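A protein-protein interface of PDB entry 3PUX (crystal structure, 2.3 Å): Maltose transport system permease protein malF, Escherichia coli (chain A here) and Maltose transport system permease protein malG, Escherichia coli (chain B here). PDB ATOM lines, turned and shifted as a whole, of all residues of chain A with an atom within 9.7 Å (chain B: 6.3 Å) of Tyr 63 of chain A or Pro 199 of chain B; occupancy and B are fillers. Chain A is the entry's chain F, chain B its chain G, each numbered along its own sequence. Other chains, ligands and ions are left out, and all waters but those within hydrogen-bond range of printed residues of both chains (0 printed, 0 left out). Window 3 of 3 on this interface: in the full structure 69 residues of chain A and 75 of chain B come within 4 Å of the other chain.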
ATOM      1  N   LYS A  16     -28.953  -1.034  -3.308  1.00  0.00           N
ATOM      2  CA  LYS A  16     -29.456  -2.154  -4.109  1.00  0.00           C
ATOM      3  C   LYS A  16     -30.457  -1.670  -5.156  1.00  0.00           C
ATOM      4  O   LYS A  16     -30.220  -1.826  -6.354  1.00  0.00           O
ATOM      5  CB  LYS A  16     -30.048  -3.286  -3.252  1.00  0.00           C
ATOM      6  CG  LYS A  16     -29.983  -4.663  -3.938  1.00  0.00           C
ATOM      7  CD  LYS A  16     -30.991  -5.658  -3.376  1.00  0.00           C
ATOM      8  CE  LYS A  16     -30.897  -7.001  -4.098  1.00  0.00           C
ATOM      9  NZ  LYS A  16     -31.810  -8.028  -3.513  1.00  0.00           N
ATOM     10  N   GLY A  53     -32.989 -11.446 -15.545  1.00  0.00           N
ATOM     11  CA  GLY A  53     -31.893 -11.078 -14.653  1.00  0.00           C
ATOM     12  C   GLY A  53     -32.289 -10.103 -13.565  1.00  0.00           C
ATOM     13  O   GLY A  53     -31.928 -10.283 -12.410  1.00  0.00           O
ATOM     14  N   TYR A  55     -35.583  -9.209 -12.466  1.00  0.00           N
ATOM     15  CA  TYR A  55     -36.635  -9.805 -11.641  1.00  0.00           C
ATOM     16  C   TYR A  55     -36.054 -10.821 -10.643  1.00  0.00           C
ATOM     17  O   TYR A  55     -36.405 -10.826  -9.466  1.00  0.00           O
ATOM     18  CB  TYR A  55     -37.708 -10.440 -12.543  1.00  0.00           C
ATOM     19  CG  TYR A  55     -38.770 -11.255 -11.826  1.00  0.00           C
ATOM     20  CD1 TYR A  55     -38.705 -12.654 -11.805  1.00  0.00           C
ATOM     21  CD2 TYR A  55     -39.838 -10.634 -11.172  1.00  0.00           C
ATOM     22  CE1 TYR A  55     -39.671 -13.410 -11.152  1.00  0.00           C
ATOM     23  CE2 TYR A  55     -40.815 -11.387 -10.508  1.00  0.00           C
ATOM     24  CZ  TYR A  55     -40.726 -12.771 -10.506  1.00  0.00           C
ATOM     25  OH  TYR A  55     -41.680 -13.527  -9.854  1.00  0.00           O
ATOM     26  N   ILE A  56     -35.158 -11.670 -11.134  1.00  0.00           N
ATOM     27  CA  ILE A  56     -34.493 -12.683 -10.317  1.00  0.00           C
ATOM     28  C   ILE A  56     -33.714 -12.065  -9.142  1.00  0.00           C
ATOM     29  O   ILE A  56     -33.751 -12.597  -8.033  1.00  0.00           O
ATOM     30  CB  ILE A  56     -33.651 -13.663 -11.211  1.00  0.00           C
ATOM     31  CG1 ILE A  56     -34.539 -14.836 -11.658  1.00  0.00           C
ATOM     32  CG2 ILE A  56     -32.351 -14.128 -10.524  1.00  0.00           C
ATOM     33  CD1 ILE A  56     -34.107 -15.508 -12.959  1.00  0.00           C
ATOM     34  N   PHE A  57     -33.041 -10.940  -9.381  1.00  0.00           N
ATOM     35  CA  PHE A  57     -32.314 -10.249  -8.318  1.00  0.00           C
ATOM     36  C   PHE A  57     -33.196  -9.266  -7.543  1.00  0.00           C
ATOM     37  O   PHE A  57     -32.766  -8.699  -6.530  1.00  0.00           O
ATOM     38  CB  PHE A  57     -31.061  -9.564  -8.870  1.00  0.00           C
ATOM     39  CG  PHE A  57     -29.890 -10.489  -9.020  1.00  0.00           C
ATOM     40  CD1 PHE A  57     -29.788 -11.335 -10.121  1.00  0.00           C
ATOM     41  CD2 PHE A  57     -28.899 -10.537  -8.045  1.00  0.00           C
ATOM     42  CE1 PHE A  57     -28.715 -12.205 -10.251  1.00  0.00           C
ATOM     43  CE2 PHE A  57     -27.818 -11.405  -8.166  1.00  0.00           C
ATOM     44  CZ  PHE A  57     -27.726 -12.238  -9.274  1.00  0.00           C
ATOM     45  N   ALA A  58     -34.435  -9.090  -8.007  1.00  0.00           N
ATOM     46  CA  ALA A  58     -35.387  -8.179  -7.374  1.00  0.00           C
ATOM     47  C   ALA A  58     -36.089  -8.824  -6.190  1.00  0.00           C
ATOM     48  O   ALA A  58     -35.917  -8.385  -5.042  1.00  0.00           O
ATOM     49  CB  ALA A  58     -36.416  -7.664  -8.389  1.00  0.00           C
ATOM     50  N   ASN A  59     -36.898  -9.846  -6.467  1.00  0.00           N
ATOM     51  CA  ASN A  59     -37.592 -10.539  -5.396  1.00  0.00           C
ATOM     52  C   ASN A  59     -36.768 -11.694  -4.857  1.00  0.00           C
ATOM     53  O   ASN A  59     -36.275 -12.544  -5.609  1.00  0.00           O
ATOM     54  CB  ASN A  59     -39.036 -10.944  -5.770  1.00  0.00           C
ATOM     55  CG  ASN A  59     -39.103 -12.046  -6.814  1.00  0.00           C
ATOM     56  OD1 ASN A  59     -39.625 -13.131  -6.546  1.00  0.00           O
ATOM     57  ND2 ASN A  59     -38.593 -11.769  -8.012  1.00  0.00           N
ATOM     58  N   ARG A  60     -36.607 -11.689  -3.538  1.00  0.00           N
ATOM     59  CA  ARG A  60     -35.779 -12.664  -2.849  1.00  0.00           C
ATOM     60  C   ARG A  60     -36.443 -14.044  -2.819  1.00  0.00           C
ATOM     61  O   ARG A  60     -35.939 -14.966  -2.182  1.00  0.00           O
ATOM     62  CB  ARG A  60     -35.419 -12.155  -1.440  1.00  0.00           C
ATOM     63  CG  ARG A  60     -34.493 -10.905  -1.429  1.00  0.00           C
ATOM     64  CD  ARG A  60     -33.042 -11.268  -1.058  1.00  0.00           C
ATOM     65  NE  ARG A  60     -32.094 -10.137  -1.086  1.00  0.00           N
ATOM     66  CZ  ARG A  60     -30.905 -10.142  -0.472  1.00  0.00           C
ATOM     67  NH1 ARG A  60     -30.514 -11.204   0.228  1.00  0.00           N
ATOM     68  NH2 ARG A  60     -30.106  -9.084  -0.548  1.00  0.00           N
ATOM     69  N   LYS A  61     -37.571 -14.183  -3.510  1.00  0.00           N
ATOM     70  CA  LYS A  61     -38.208 -15.493  -3.660  1.00  0.00           C
ATOM     71  C   LYS A  61     -37.584 -16.310  -4.791  1.00  0.00           C
ATOM     72  O   LYS A  61     -37.677 -17.539  -4.806  1.00  0.00           O
ATOM     73  CB  LYS A  61     -39.739 -15.392  -3.776  1.00  0.00           C
ATOM     74  CG  LYS A  61     -40.443 -15.804  -2.472  1.00  0.00           C
ATOM     75  CD  LYS A  61     -41.893 -15.336  -2.345  1.00  0.00           C
ATOM     76  CE  LYS A  61     -42.493 -15.911  -1.053  1.00  0.00           C
ATOM     77  NZ  LYS A  61     -43.852 -15.382  -0.708  1.00  0.00           N
ATOM     78  N   ALA A  62     -36.920 -15.625  -5.716  1.00  0.00           N
ATOM     79  CA  ALA A  62     -36.197 -16.300  -6.777  1.00  0.00           C
ATOM     80  C   ALA A  62     -34.701 -16.421  -6.440  1.00  0.00           C
ATOM     81  O   ALA A  62     -33.862 -16.414  -7.333  1.00  0.00           O
ATOM     82  CB  ALA A  62     -36.420 -15.590  -8.094  1.00  0.00           C
ATOM     83  N   TYR A  63     -34.392 -16.562  -5.145  1.00  0.00           N
ATOM     84  CA  TYR A  63     -33.011 -16.636  -4.632  1.00  0.00           C
ATOM     85  C   TYR A  63     -32.128 -17.612  -5.388  1.00  0.00           C
ATOM     86  O   TYR A  63     -31.162 -17.206  -6.035  1.00  0.00           O
ATOM     87  CB  TYR A  63     -32.990 -16.996  -3.141  1.00  0.00           C
ATOM     88  CG  TYR A  63     -31.619 -16.852  -2.503  1.00  0.00           C
ATOM     89  CD1 TYR A  63     -30.817 -17.971  -2.237  1.00  0.00           C
ATOM     90  CD2 TYR A  63     -31.118 -15.595  -2.174  1.00  0.00           C
ATOM     91  CE1 TYR A  63     -29.551 -17.833  -1.640  1.00  0.00           C
ATOM     92  CE2 TYR A  63     -29.862 -15.445  -1.584  1.00  0.00           C
ATOM     93  CZ  TYR A  63     -29.082 -16.562  -1.314  1.00  0.00           C
ATOM     94  OH  TYR A  63     -27.844 -16.385  -0.723  1.00  0.00           O
ATOM     95  N   ALA A  64     -32.474 -18.893  -5.329  1.00  0.00           N
ATOM     96  CA  ALA A  64     -31.649 -19.929  -5.954  1.00  0.00           C
ATOM     97  C   ALA A  64     -31.266 -19.631  -7.407  1.00  0.00           C
ATOM     98  O   ALA A  64     -30.161 -19.960  -7.827  1.00  0.00           O
ATOM     99  CB  ALA A  64     -32.315 -21.299  -5.834  1.00  0.00           C
ATOM    100  N   TRP A  65     -32.163 -18.999  -8.159  1.00  0.00           N
ATOM    101  CA  TRP A  65     -31.918 -18.658  -9.555  1.00  0.00           C
ATOM    102  C   TRP A  65     -30.764 -17.690  -9.730  1.00  0.00           C
ATOM    103  O   TRP A  65     -30.134 -17.682 -10.770  1.00  0.00           O
ATOM    104  CB  TRP A  65     -33.181 -18.094 -10.198  1.00  0.00           C
ATOM    105  CG  TRP A  65     -34.276 -19.084 -10.212  1.00  0.00           C
ATOM    106  CD1 TRP A  65     -35.262 -19.249  -9.267  1.00  0.00           C
ATOM    107  CD2 TRP A  65     -34.486 -20.095 -11.194  1.00  0.00           C
ATOM    108  NE1 TRP A  65     -36.084 -20.296  -9.621  1.00  0.00           N
ATOM    109  CE2 TRP A  65     -35.631 -20.829 -10.800  1.00  0.00           C
ATOM    110  CE3 TRP A  65     -33.825 -20.446 -12.377  1.00  0.00           C
ATOM    111  CZ2 TRP A  65     -36.125 -21.901 -11.551  1.00  0.00           C
ATOM    112  CZ3 TRP A  65     -34.317 -21.507 -13.128  1.00  0.00           C
ATOM    113  CH2 TRP A  65     -35.457 -22.224 -12.709  1.00  0.00           C
ATOM    114  N   ARG A  66     -30.494 -16.880  -8.710  1.00  0.00           N
ATOM    115  CA  ARG A  66     -29.334 -15.988  -8.673  1.00  0.00           C
ATOM    116  C   ARG A  66     -28.034 -16.714  -8.964  1.00  0.00           C
ATOM    117  O   ARG A  66     -27.108 -16.146  -9.542  1.00  0.00           O
ATOM    118  CB  ARG A  66     -29.214 -15.330  -7.303  1.00  0.00           C
ATOM    119  CG  ARG A  66     -30.282 -14.277  -7.083  1.00  0.00           C
ATOM    120  CD  ARG A  66     -30.179 -13.539  -5.758  1.00  0.00           C
ATOM    121  NE  ARG A  66     -31.435 -12.818  -5.550  1.00  0.00           N
ATOM    122  CZ  ARG A  66     -31.739 -12.070  -4.492  1.00  0.00           C
ATOM    123  NH1 ARG A  66     -30.868 -11.907  -3.498  1.00  0.00           N
ATOM    124  NH2 ARG A  66     -32.927 -11.473  -4.445  1.00  0.00           N
ATOM    125  N   TYR A  67     -27.982 -17.974  -8.546  1.00  0.00           N
ATOM    126  CA  TYR A  67     -26.798 -18.806  -8.682  1.00  0.00           C
ATOM    127  C   TYR A  67     -26.761 -19.467 -10.045  1.00  0.00           C
ATOM    128  O   TYR A  67     -25.685 -19.721 -10.596  1.00  0.00           O
ATOM    129  CB  TYR A  67     -26.785 -19.865  -7.579  1.00  0.00           C
ATOM    130  CG  TYR A  67     -26.473 -19.327  -6.199  1.00  0.00           C
ATOM    131  CD1 TYR A  67     -27.455 -18.714  -5.424  1.00  0.00           C
ATOM    132  CD2 TYR A  67     -25.190 -19.447  -5.662  1.00  0.00           C
ATOM    133  CE1 TYR A  67     -27.155 -18.226  -4.169  1.00  0.00           C
ATOM    134  CE2 TYR A  67     -24.887 -18.960  -4.394  1.00  0.00           C
ATOM    135  CZ  TYR A  67     -25.860 -18.353  -3.667  1.00  0.00           C
ATOM    136  OH  TYR A  67     -25.550 -17.884  -2.419  1.00  0.00           O
ATOM    137  N   VAL A  68     -27.934 -19.718 -10.604  1.00  0.00           N
ATOM    138  CA  VAL A  68     -28.045 -20.456 -11.856  1.00  0.00           C
ATOM    139  C   VAL A  68     -27.997 -19.539 -13.075  1.00  0.00           C
ATOM    140  O   VAL A  68     -27.501 -19.911 -14.154  1.00  0.00           O
ATOM    141  CB  VAL A  68     -29.360 -21.248 -11.889  1.00  0.00           C
ATOM    142  CG1 VAL A  68     -29.224 -22.416 -12.785  1.00  0.00           C
ATOM    143  CG2 VAL A  68     -29.673 -21.762 -10.513  1.00  0.00           C
ATOM    144  N   TYR A  69     -28.529 -18.336 -12.895  1.00  0.00           N
ATOM    145  CA  TYR A  69     -28.832 -17.463 -14.011  1.00  0.00           C
ATOM    146  C   TYR A  69     -27.611 -17.030 -14.811  1.00  0.00           C
ATOM    147  O   TYR A  69     -27.649 -17.126 -16.034  1.00  0.00           O
ATOM    148  CB  TYR A  69     -29.656 -16.260 -13.561  1.00  0.00           C
ATOM    149  CG  TYR A  69     -29.669 -15.150 -14.563  1.00  0.00           C
ATOM    150  CD1 TYR A  69     -28.714 -14.128 -14.500  1.00  0.00           C
ATOM    151  CD2 TYR A  69     -30.620 -15.119 -15.577  1.00  0.00           C
ATOM    152  CE1 TYR A  69     -28.696 -13.102 -15.417  1.00  0.00           C
ATOM    153  CE2 TYR A  69     -30.619 -14.097 -16.508  1.00  0.00           C
ATOM    154  CZ  TYR A  69     -29.649 -13.086 -16.423  1.00  0.00           C
ATOM    155  OH  TYR A  69     -29.637 -12.051 -17.336  1.00  0.00           O
ATOM    156  N   PRO A  70     -26.536 -16.549 -14.139  1.00  0.00           N
ATOM    157  CA  PRO A  70     -25.309 -16.211 -14.884  1.00  0.00           C
ATOM    158  C   PRO A  70     -24.836 -17.363 -15.768  1.00  0.00           C
ATOM    159  O   PRO A  70     -24.536 -17.161 -16.948  1.00  0.00           O
ATOM    160  CB  PRO A  70     -24.288 -15.933 -13.773  1.00  0.00           C
ATOM    161  CG  PRO A  70     -25.129 -15.521 -12.592  1.00  0.00           C
ATOM    162  CD  PRO A  70     -26.369 -16.336 -12.687  1.00  0.00           C
ATOM    163  N   TYR B 108     -23.681 -25.290  -6.838  1.00  0.00           N
ATOM    164  CA  TYR B 108     -24.211 -25.037  -5.503  1.00  0.00           C
ATOM    165  C   TYR B 108     -25.733 -25.090  -5.505  1.00  0.00           C
ATOM    166  O   TYR B 108     -26.323 -25.845  -4.739  1.00  0.00           O
ATOM    167  CB  TYR B 108     -23.679 -23.706  -4.965  1.00  0.00           C
ATOM    168  CG  TYR B 108     -24.071 -23.406  -3.557  1.00  0.00           C
ATOM    169  CD1 TYR B 108     -23.815 -24.312  -2.525  1.00  0.00           C
ATOM    170  CD2 TYR B 108     -24.682 -22.214  -3.233  1.00  0.00           C
ATOM    171  CE1 TYR B 108     -24.190 -24.033  -1.214  1.00  0.00           C
ATOM    172  CE2 TYR B 108     -25.070 -21.927  -1.909  1.00  0.00           C
ATOM    173  CZ  TYR B 108     -24.819 -22.838  -0.914  1.00  0.00           C
ATOM    174  OH  TYR B 108     -25.180 -22.549   0.384  1.00  0.00           O
ATOM    175  N   MET B 113     -29.933 -26.435  -3.172  1.00  0.00           N
ATOM    176  CA  MET B 113     -31.193 -25.716  -3.205  1.00  0.00           C
ATOM    177  C   MET B 113     -32.175 -26.481  -4.059  1.00  0.00           C
ATOM    178  O   MET B 113     -31.792 -27.391  -4.792  1.00  0.00           O
ATOM    179  CB  MET B 113     -30.968 -24.305  -3.747  1.00  0.00           C
ATOM    180  CG  MET B 113     -29.924 -23.529  -2.944  1.00  0.00           C
ATOM    181  SD  MET B 113     -29.398 -21.984  -3.697  1.00  0.00           S
ATOM    182  CE  MET B 113     -28.386 -21.315  -2.392  1.00  0.00           C
ATOM    183  N   ALA B 197     -25.343 -18.181   9.355  1.00  0.00           N
ATOM    184  CA  ALA B 197     -24.705 -17.962   8.071  1.00  0.00           C
ATOM    185  C   ALA B 197     -25.749 -18.002   6.978  1.00  0.00           C
ATOM    186  O   ALA B 197     -26.652 -18.834   6.998  1.00  0.00           O
ATOM    187  CB  ALA B 197     -23.630 -18.984   7.808  1.00  0.00           C
ATOM    188  N   THR B 198     -25.623 -17.081   6.034  1.00  0.00           N
ATOM    189  CA  THR B 198     -26.502 -17.027   4.871  1.00  0.00           C
ATOM    190  C   THR B 198     -26.137 -18.176   3.937  1.00  0.00           C
ATOM    191  O   THR B 198     -25.068 -18.748   4.068  1.00  0.00           O
ATOM    192  CB  THR B 198     -26.325 -15.714   4.118  1.00  0.00           C
ATOM    193  OG1 THR B 198     -24.960 -15.607   3.688  1.00  0.00           O
ATOM    194  CG2 THR B 198     -26.682 -14.532   5.004  1.00  0.00           C
ATOM    195  N   PRO B 199     -27.025 -18.518   2.989  1.00  0.00           N
ATOM    196  CA  PRO B 199     -26.605 -19.534   2.014  1.00  0.00           C
ATOM    197  C   PRO B 199     -25.295 -19.154   1.300  1.00  0.00           C
ATOM    198  O   PRO B 199     -24.445 -20.035   1.060  1.00  0.00           O
ATOM    199  CB  PRO B 199     -27.792 -19.575   1.033  1.00  0.00           C
ATOM    200  CG  PRO B 199     -28.980 -19.185   1.906  1.00  0.00           C
ATOM    201  CD  PRO B 199     -28.417 -18.086   2.762  1.00  0.00           C
ATOM    202  N   TRP B 200     -25.110 -17.868   1.003  1.00  0.00           N
ATOM    203  CA  TRP B 200     -23.858 -17.406   0.393  1.00  0.00           C
ATOM    204  C   TRP B 200     -22.637 -17.657   1.299  1.00  0.00           C
ATOM    205  O   TRP B 200     -21.608 -18.134   0.835  1.00  0.00           O
ATOM    206  CB  TRP B 200     -23.908 -15.921  -0.049  1.00  0.00           C
ATOM    207  CG  TRP B 200     -22.532 -15.440  -0.500  1.00  0.00           C
ATOM    208  CD1 TRP B 200     -21.589 -14.796   0.266  1.00  0.00           C
ATOM    209  CD2 TRP B 200     -21.923 -15.645  -1.788  1.00  0.00           C
ATOM    210  NE1 TRP B 200     -20.445 -14.565  -0.471  1.00  0.00           N
ATOM    211  CE2 TRP B 200     -20.619 -15.075  -1.732  1.00  0.00           C
ATOM    212  CE3 TRP B 200     -22.354 -16.237  -2.983  1.00  0.00           C
ATOM    213  CZ2 TRP B 200     -19.741 -15.087  -2.820  1.00  0.00           C
ATOM    214  CZ3 TRP B 200     -21.478 -16.242  -4.084  1.00  0.00           C
ATOM    215  CH2 TRP B 200     -20.184 -15.668  -3.987  1.00  0.00           C
ATOM    216  N   GLN B 201     -22.768 -17.309   2.577  1.00  0.00           N
ATOM    217  CA  GLN B 201     -21.716 -17.474   3.571  1.00  0.00           C
ATOM    218  C   GLN B 201     -21.359 -18.932   3.774  1.00  0.00           C
ATOM    219  O   GLN B 201     -20.190 -19.259   3.975  1.00  0.00           O
ATOM    220  CB  GLN B 201     -22.148 -16.841   4.906  1.00  0.00           C
ATOM    221  CG  GLN B 201     -21.928 -15.314   4.939  1.00  0.00           C
ATOM    222  CD  GLN B 201     -22.679 -14.591   6.050  1.00  0.00           C
ATOM    223  OE1 GLN B 201     -23.648 -15.095   6.631  1.00  0.00           O
ATOM    224  NE2 GLN B 201     -22.246 -13.377   6.330  1.00  0.00           N
ATOM    225  N   ALA B 202     -22.369 -19.803   3.716  1.00  0.00           N
ATOM    226  CA  ALA B 202     -22.173 -21.237   3.934  1.00  0.00           C
ATOM    227  C   ALA B 202     -21.359 -21.752   2.768  1.00  0.00           C
ATOM    228  O   ALA B 202     -20.374 -22.485   2.951  1.00  0.00           O
ATOM    229  CB  ALA B 202     -23.508 -21.956   4.034  1.00  0.00           C
ATOM    230  N   PHE B 203     -21.769 -21.323   1.578  1.00  0.00           N
ATOM    231  CA  PHE B 203     -21.074 -21.574   0.325  1.00  0.00           C
ATOM    232  C   PHE B 203     -19.611 -21.144   0.393  1.00  0.00           C
ATOM    233  O   PHE B 203     -18.733 -21.963   0.253  1.00  0.00           O
ATOM    234  CB  PHE B 203     -21.824 -20.890  -0.805  1.00  0.00           C
ATOM    235  CG  PHE B 203     -21.150 -20.961  -2.139  1.00  0.00           C
ATOM    236  CD1 PHE B 203     -20.684 -19.807  -2.745  1.00  0.00           C
ATOM    237  CD2 PHE B 203     -21.020 -22.176  -2.822  1.00  0.00           C
ATOM    238  CE1 PHE B 203     -20.066 -19.849  -4.012  1.00  0.00           C
ATOM    239  CE2 PHE B 203     -20.417 -22.233  -4.085  1.00  0.00           C
ATOM    240  CZ  PHE B 203     -19.934 -21.073  -4.677  1.00  0.00           C
ATOM    241  N   ARG B 204     -19.360 -19.874   0.665  1.00  0.00           N
ATOM    242  CA  ARG B 204     -17.992 -19.334   0.667  1.00  0.00           C
ATOM    243  C   ARG B 204     -17.122 -19.824   1.815  1.00  0.00           C
ATOM    244  O   ARG B 204     -15.961 -20.157   1.613  1.00  0.00           O
ATOM    245  CB  ARG B 204     -18.028 -17.796   0.684  1.00  0.00           C
ATOM    246  CG  ARG B 204     -16.775 -17.107   0.114  1.00  0.00           C
ATOM    247  CD  ARG B 204     -16.520 -15.820   0.884  1.00  0.00           C
ATOM    248  NE  ARG B 204     -15.455 -14.966   0.338  1.00  0.00           N
ATOM    249  CZ  ARG B 204     -15.072 -13.811   0.897  1.00  0.00           C
ATOM    250  NH1 ARG B 204     -15.648 -13.380   2.022  1.00  0.00           N
ATOM    251  NH2 ARG B 204     -14.103 -13.082   0.349  1.00  0.00           N
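The side-chain hydroxyl of Tyr 67 of chain A lies close to the backbone NH of Trp 200 of chain B, at 3.5 Å.
OH of Tyr 67 of chain A lies within hydrogen-bond range of OH of Tyr 63 of chain A, at 3.2 Å. The backbone carbonyl oxygen (O) of Pro 199 of chain B is in hydrogen-bond range of the side-chain hydroxyl (OH) of Tyr 108 of chain B (2.7 Å).
Among the printed residues, merely in contact across the chains: Tyr 67 of chain A with Tyr 108 of chain B (3.5 Å), Tyr 63 of chain A with Trp 200 of chain B (3.6 Å), Tyr 63 of chain A with Pro 199 of chain B (3.6 Å), Ala 64 of chain A with Met 113 of chain B (3.7 Å), Tyr 63 of chain A with Met 113 of chain B (3.7 Å), Tyr 67 of chain A with Met 113 of chain B (3.8 Å) and Tyr 67 of chain A with Pro 199 of chain B (3.9 Å).
Of chain B, only Met 113, Pro 199 and Trp 200 come within 4 Å of Tyr 63 of chain A. Printed residues of chain B within 4 Å of Ala 64 of chain A: Met 113 (3.7 Å). Of the printed residues of chain B, Tyr 67 of chain A touches Tyr 108, Met 113, Pro 199 and Trp 200. Of the printed residues of chain A, Tyr 108 of chain B touches Tyr 67 (3.5 Å). Thr 198 of chain B touches none of the printed residues of chain A. Pro 199 of chain B touches just these residues of chain A: Tyr 63 and Tyr 67. Of the printed residues of chain A, Trp 200 of chain B touches Tyr 63 (3.6 Å) and Tyr 67 (3.3 Å). Ala 202 of chain B touches none of the printed residues of chain A. The nearest residue of chain B that does not touch Tyr 63 of chain A is Thr 198 of chain B (5.1 Å). The nearest printed residue of chain A that does not touch Trp 200 of chain B is Arg 66 of chain A (7.8 Å).
Of the 10 printed residues of chain B, 4 touch a printed residue of chain A. Hydrophobic or aromatic side chains of chain B that line the printed part of chain A: Tyr 108, Met 113, Pro 199 and Trp 200. Hydrophobic or aromatic side chains of chain A within 4 Å of the printed part of chain B: Tyr 63, Ala 64 and Tyr 67. Among the printed residues, 8 pairs touch across the chains. Among the printed residues, no Asp or Glu carboxylate lies within 4 Å of a Lys or Arg side-chain nitrogen of the other chain.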
